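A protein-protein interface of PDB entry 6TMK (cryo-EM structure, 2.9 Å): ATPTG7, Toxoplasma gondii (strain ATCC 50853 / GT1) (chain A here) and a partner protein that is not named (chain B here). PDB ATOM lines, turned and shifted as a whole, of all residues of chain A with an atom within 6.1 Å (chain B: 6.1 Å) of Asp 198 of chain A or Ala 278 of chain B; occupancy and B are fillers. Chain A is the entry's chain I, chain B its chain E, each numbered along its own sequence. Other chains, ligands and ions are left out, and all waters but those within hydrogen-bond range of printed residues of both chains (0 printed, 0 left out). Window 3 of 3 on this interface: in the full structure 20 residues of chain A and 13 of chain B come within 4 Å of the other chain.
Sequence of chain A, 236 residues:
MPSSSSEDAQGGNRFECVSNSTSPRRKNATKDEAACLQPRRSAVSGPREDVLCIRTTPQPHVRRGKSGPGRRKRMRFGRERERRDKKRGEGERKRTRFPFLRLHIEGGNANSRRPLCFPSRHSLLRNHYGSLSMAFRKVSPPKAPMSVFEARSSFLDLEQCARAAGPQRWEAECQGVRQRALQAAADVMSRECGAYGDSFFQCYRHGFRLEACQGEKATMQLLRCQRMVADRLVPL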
ATOM      1  N   CYS A 193      14.394  -6.203   7.485  1.00  0.00           N
ATOM      2  CA  CYS A 193      13.713  -4.962   7.136  1.00  0.00           C
ATOM      3  C   CYS A 193      14.691  -3.805   6.976  1.00  0.00           C
ATOM      4  O   CYS A 193      14.275  -2.644   7.000  1.00  0.00           O
ATOM      5  CB  CYS A 193      12.661  -4.617   8.192  1.00  0.00           C
ATOM      6  SG  CYS A 193      11.569  -5.980   8.662  1.00  0.00           S
ATOM      7  N   GLY A 194      15.980  -4.097   6.810  1.00  0.00           N
ATOM      8  CA  GLY A 194      16.968  -3.043   6.672  1.00  0.00           C
ATOM      9  C   GLY A 194      16.934  -2.348   5.328  1.00  0.00           C
ATOM     10  O   GLY A 194      17.202  -1.146   5.242  1.00  0.00           O
ATOM     11  N   ALA A 195      16.618  -3.083   4.264  1.00  0.00           N
ATOM     12  CA  ALA A 195      16.507  -2.470   2.946  1.00  0.00           C
ATOM     13  C   ALA A 195      15.421  -1.404   2.919  1.00  0.00           C
ATOM     14  O   ALA A 195      15.624  -0.310   2.378  1.00  0.00           O
ATOM     15  CB  ALA A 195      16.222  -3.541   1.897  1.00  0.00           C
ATOM     16  N   TYR A 196      14.268  -1.695   3.515  1.00  0.00           N
ATOM     17  CA  TYR A 196      13.174  -0.734   3.522  1.00  0.00           C
ATOM     18  C   TYR A 196      13.510   0.477   4.382  1.00  0.00           C
ATOM     19  O   TYR A 196      13.151   1.610   4.039  1.00  0.00           O
ATOM     20  CB  TYR A 196      11.906  -1.410   4.025  1.00  0.00           C
ATOM     21  CG  TYR A 196      11.416  -2.525   3.140  1.00  0.00           C
ATOM     22  CD1 TYR A 196      11.026  -2.285   1.835  1.00  0.00           C
ATOM     23  CD2 TYR A 196      11.348  -3.823   3.612  1.00  0.00           C
ATOM     24  CE1 TYR A 196      10.579  -3.306   1.029  1.00  0.00           C
ATOM     25  CE2 TYR A 196      10.905  -4.846   2.815  1.00  0.00           C
ATOM     26  CZ  TYR A 196      10.520  -4.584   1.526  1.00  0.00           C
ATOM     27  OH  TYR A 196      10.078  -5.614   0.737  1.00  0.00           O
ATOM     28  N   GLY A 197      14.197   0.259   5.500  1.00  0.00           N
ATOM     29  CA  GLY A 197      14.622   1.377   6.319  1.00  0.00           C
ATOM     30  C   GLY A 197      15.623   2.267   5.611  1.00  0.00           C
ATOM     31  O   GLY A 197      15.545   3.494   5.691  1.00  0.00           O
ATOM     32  N   ASP A 198      16.576   1.661   4.905  1.00  0.00           N
ATOM     33  CA  ASP A 198      17.526   2.443   4.125  1.00  0.00           C
ATOM     34  C   ASP A 198      16.827   3.201   3.004  1.00  0.00           C
ATOM     35  O   ASP A 198      17.202   4.333   2.683  1.00  0.00           O
ATOM     36  CB  ASP A 198      18.611   1.527   3.565  1.00  0.00           C
ATOM     37  CG  ASP A 198      19.477   0.922   4.646  1.00  0.00           C
ATOM     38  OD1 ASP A 198      19.880  -0.249   4.499  1.00  0.00           O
ATOM     39  OD2 ASP A 198      19.758   1.615   5.644  1.00  0.00           O
ATOM     40  N   SER A 199      15.798   2.600   2.407  1.00  0.00           N
ATOM     41  CA  SER A 199      15.058   3.289   1.356  1.00  0.00           C
ATOM     42  C   SER A 199      14.302   4.485   1.914  1.00  0.00           C
ATOM     43  O   SER A 199      14.280   5.558   1.299  1.00  0.00           O
ATOM     44  CB  SER A 199      14.100   2.320   0.669  1.00  0.00           C
ATOM     45  OG  SER A 199      14.807   1.358  -0.084  1.00  0.00           O
ATOM     46  N   PHE A 200      13.669   4.320   3.075  1.00  0.00           N
ATOM     47  CA  PHE A 200      13.012   5.448   3.719  1.00  0.00           C
ATOM     48  C   PHE A 200      14.015   6.538   4.070  1.00  0.00           C
ATOM     49  O   PHE A 200      13.737   7.728   3.891  1.00  0.00           O
ATOM     50  CB  PHE A 200      12.277   4.995   4.975  1.00  0.00           C
ATOM     51  CG  PHE A 200      11.533   6.096   5.654  1.00  0.00           C
ATOM     52  CD1 PHE A 200      10.254   6.419   5.263  1.00  0.00           C
ATOM     53  CD2 PHE A 200      12.121   6.832   6.660  1.00  0.00           C
ATOM     54  CE1 PHE A 200       9.574   7.431   5.870  1.00  0.00           C
ATOM     55  CE2 PHE A 200      11.443   7.853   7.266  1.00  0.00           C
ATOM     56  CZ  PHE A 200      10.170   8.152   6.870  1.00  0.00           C
ATOM     57  N   PHE A 201      15.169   6.151   4.610  1.00  0.00           N
ATOM     58  CA  PHE A 201      16.219   7.114   4.918  1.00  0.00           C
ATOM     59  C   PHE A 201      16.625   7.901   3.678  1.00  0.00           C
ATOM     60  O   PHE A 201      16.788   9.127   3.730  1.00  0.00           O
ATOM     61  CB  PHE A 201      17.413   6.378   5.512  1.00  0.00           C
ATOM     62  CG  PHE A 201      18.536   7.270   5.907  1.00  0.00           C
ATOM     63  CD1 PHE A 201      18.419   8.098   7.001  1.00  0.00           C
ATOM     64  CD2 PHE A 201      19.717   7.273   5.195  1.00  0.00           C
ATOM     65  CE1 PHE A 201      19.444   8.912   7.371  1.00  0.00           C
ATOM     66  CE2 PHE A 201      20.747   8.091   5.565  1.00  0.00           C
ATOM     67  CZ  PHE A 201      20.610   8.910   6.656  1.00  0.00           C
ATOM     68  N   GLN A 202      16.801   7.209   2.555  1.00  0.00           N
ATOM     69  CA  GLN A 202      17.209   7.870   1.324  1.00  0.00           C
ATOM     70  C   GLN A 202      16.134   8.838   0.850  1.00  0.00           C
ATOM     71  O   GLN A 202      16.429   9.971   0.450  1.00  0.00           O
ATOM     72  CB  GLN A 202      17.499   6.813   0.265  1.00  0.00           C
ATOM     73  CG  GLN A 202      18.168   7.317  -0.986  1.00  0.00           C
ATOM     74  CD  GLN A 202      19.578   7.793  -0.736  1.00  0.00           C
ATOM     75  OE1 GLN A 202      19.963   8.888  -1.137  1.00  0.00           O
ATOM     76  NE2 GLN A 202      20.358   6.968  -0.067  1.00  0.00           N
ATOM     77  N   CYS A 203      14.878   8.397   0.872  1.00  0.00           N
ATOM     78  CA  CYS A 203      13.780   9.278   0.503  1.00  0.00           C
ATOM     79  C   CYS A 203      13.723  10.503   1.406  1.00  0.00           C
ATOM     80  O   CYS A 203      13.452  11.616   0.943  1.00  0.00           O
ATOM     81  CB  CYS A 203      12.467   8.503   0.568  1.00  0.00           C
ATOM     82  SG  CYS A 203      12.205   7.359  -0.786  1.00  0.00           S
ATOM     83  N   GLY B 263      27.194  -2.439   0.294  1.00  0.00           N
ATOM     84  CA  GLY B 263      26.002  -1.995   0.987  1.00  0.00           C
ATOM     85  C   GLY B 263      24.961  -3.072   1.191  1.00  0.00           C
ATOM     86  O   GLY B 263      24.074  -2.908   2.035  1.00  0.00           O
ATOM     87  N   ARG B 274      28.155   1.496   3.729  1.00  0.00           N
ATOM     88  CA  ARG B 274      27.092   2.418   4.075  1.00  0.00           C
ATOM     89  C   ARG B 274      27.696   3.356   5.103  1.00  0.00           C
ATOM     90  O   ARG B 274      28.921   3.464   5.207  1.00  0.00           O
ATOM     91  CB  ARG B 274      25.864   1.691   4.611  1.00  0.00           C
ATOM     92  CG  ARG B 274      25.294   0.678   3.654  1.00  0.00           C
ATOM     93  CD  ARG B 274      23.949   0.161   4.115  1.00  0.00           C
ATOM     94  NE  ARG B 274      24.012  -0.493   5.415  1.00  0.00           N
ATOM     95  CZ  ARG B 274      24.304  -1.775   5.596  1.00  0.00           C
ATOM     96  NH1 ARG B 274      24.336  -2.276   6.817  1.00  0.00           N
ATOM     97  NH2 ARG B 274      24.568  -2.558   4.564  1.00  0.00           N
ATOM     98  N   GLY B 275      26.857   4.050   5.864  1.00  0.00           N
ATOM     99  CA  GLY B 275      27.293   5.143   6.695  1.00  0.00           C
ATOM    100  C   GLY B 275      26.929   4.947   8.156  1.00  0.00           C
ATOM    101  O   GLY B 275      26.153   4.060   8.526  1.00  0.00           O
ATOM    102  N   ALA B 276      27.521   5.801   8.990  1.00  0.00           N
ATOM    103  CA  ALA B 276      27.107   5.893  10.378  1.00  0.00           C
ATOM    104  C   ALA B 276      25.717   6.493  10.511  1.00  0.00           C
ATOM    105  O   ALA B 276      25.027   6.217  11.496  1.00  0.00           O
ATOM    106  CB  ALA B 276      28.119   6.723  11.162  1.00  0.00           C
ATOM    107  N   ALA B 277      25.286   7.287   9.532  1.00  0.00           N
ATOM    108  CA  ALA B 277      23.952   7.868   9.581  1.00  0.00           C
ATOM    109  C   ALA B 277      22.890   6.796   9.386  1.00  0.00           C
ATOM    110  O   ALA B 277      21.905   6.732  10.131  1.00  0.00           O
ATOM    111  CB  ALA B 277      23.822   8.953   8.521  1.00  0.00           C
ATOM    112  N   ALA B 278      23.071   5.949   8.373  1.00  0.00           N
ATOM    113  CA  ALA B 278      22.147   4.848   8.146  1.00  0.00           C
ATOM    114  C   ALA B 278      22.146   3.881   9.319  1.00  0.00           C
ATOM    115  O   ALA B 278      21.090   3.381   9.722  1.00  0.00           O
ATOM    116  CB  ALA B 278      22.516   4.127   6.858  1.00  0.00           C
ATOM    117  N   THR B 279      23.323   3.598   9.879  1.00  0.00           N
ATOM    118  CA  THR B 279      23.399   2.694  11.019  1.00  0.00           C
ATOM    119  C   THR B 279      22.688   3.283  12.228  1.00  0.00           C
ATOM    120  O   THR B 279      21.991   2.570  12.959  1.00  0.00           O
ATOM    121  CB  THR B 279      24.863   2.394  11.342  1.00  0.00           C
ATOM    122  OG1 THR B 279      25.548   1.999  10.152  1.00  0.00           O
ATOM    123  CG2 THR B 279      24.976   1.290  12.372  1.00  0.00           C
ATOM    124  N   ALA B 280      22.846   4.587  12.451  1.00  0.00           N
ATOM    125  CA  ALA B 280      22.152   5.242  13.549  1.00  0.00           C
ATOM    126  C   ALA B 280      20.644   5.219  13.345  1.00  0.00           C
ATOM    127  O   ALA B 280      19.884   4.980  14.290  1.00  0.00           O
ATOM    128  CB  ALA B 280      22.650   6.675  13.678  1.00  0.00           C
ATOM    129  N   PHE B 281      20.192   5.479  12.119  1.00  0.00           N
ATOM    130  CA  PHE B 281      18.769   5.393  11.812  1.00  0.00           C
ATOM    131  C   PHE B 281      18.237   3.995  12.084  1.00  0.00           C
ATOM    132  O   PHE B 281      17.148   3.826  12.650  1.00  0.00           O
ATOM    133  CB  PHE B 281      18.548   5.799  10.361  1.00  0.00           C
ATOM    134  CG  PHE B 281      17.117   5.790   9.937  1.00  0.00           C
ATOM    135  CD1 PHE B 281      16.233   6.724  10.428  1.00  0.00           C
ATOM    136  CD2 PHE B 281      16.663   4.867   9.022  1.00  0.00           C
ATOM    137  CE1 PHE B 281      14.927   6.719  10.037  1.00  0.00           C
ATOM    138  CE2 PHE B 281      15.354   4.862   8.628  1.00  0.00           C
ATOM    139  CZ  PHE B 281      14.486   5.792   9.131  1.00  0.00           C
ATOM    140  N   ARG B 282      18.992   2.979  11.674  1.00  0.00           N
ATOM    141  CA  ARG B 282      18.603   1.599  11.922  1.00  0.00           C
ATOM    142  C   ARG B 282      18.506   1.317  13.414  1.00  0.00           C
ATOM    143  O   ARG B 282      17.577   0.645  13.869  1.00  0.00           O
ATOM    144  CB  ARG B 282      19.609   0.669  11.257  1.00  0.00           C
ATOM    145  CG  ARG B 282      19.153  -0.747  11.097  1.00  0.00           C
ATOM    146  CD  ARG B 282      20.175  -1.530  10.323  1.00  0.00           C
ATOM    147  NE  ARG B 282      20.142  -1.187   8.907  1.00  0.00           N
ATOM    148  CZ  ARG B 282      20.522  -2.004   7.932  1.00  0.00           C
ATOM    149  NH1 ARG B 282      20.972  -3.216   8.211  1.00  0.00           N
ATOM    150  NH2 ARG B 282      20.451  -1.605   6.673  1.00  0.00           N
ATOM    151  N   ALA B 283      19.450   1.844  14.194  1.00  0.00           N
ATOM    152  CA  ALA B 283      19.412   1.658  15.639  1.00  0.00           C
ATOM    153  C   ALA B 283      18.203   2.348  16.261  1.00  0.00           C
ATOM    154  O   ALA B 283      17.603   1.831  17.211  1.00  0.00           O
ATOM    155  CB  ALA B 283      20.697   2.189  16.254  1.00  0.00           C
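NH2 of Arg 282 of chain B lies within salt-bridge range of OD1 of Asp 198 of chain A, 2.6 Å away.
Among the printed residues, pairs that only touch across the chains: Gly 194 of chain A with Arg 282 of chain B (3.6 Å), Gly 197 of chain A with Phe 281 of chain B (3.2 Å), Asp 198 of chain A with Ala 278 of chain B (3.9 Å), Phe 200 of chain A with Phe 281 of chain B (3.6 Å), Phe 201 of chain A with Ala 277 of chain B (3.7 Å) and Phe 201 of chain A with Phe 281 of chain B (3.9 Å).
Ala 195 of chain A touches none of the printed residues of chain B.
Asp 198 of chain A touches just these residues of chain B: Ala 278 and Arg 282.
Printed residues of chain B within 4 Å of Phe 201 of chain A: Ala 277 and Phe 281.
Cys 203 of chain A touches none of the printed residues of chain B.
Ala 278 of chain B touches one residue of chain A.
Of the printed residues of chain A, Phe 281 of chain B touches Gly 197, Phe 200 and Phe 201.
The nearest residue of chain A that does not touch Ala 278 of chain B is Phe 201 of chain A (4.2 Å).
The nearest printed residue of chain B that does not touch Gly 194 of chain A is Arg 274 of chain B (6.8 Å).
Hydrophobic or aromatic side chains of chain B within 4 Å of the printed part of chain A: Ala 277, Ala 278 and Phe 281.
Among the printed residues, 7 pairs touch across the chains.
Among the printed residues, Asp or Glu carboxylates within 4 Å of a Lys or Arg side-chain nitrogen of the other chain: Asp 198 of chain A with Arg 282 of chain B (2.6 Å).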
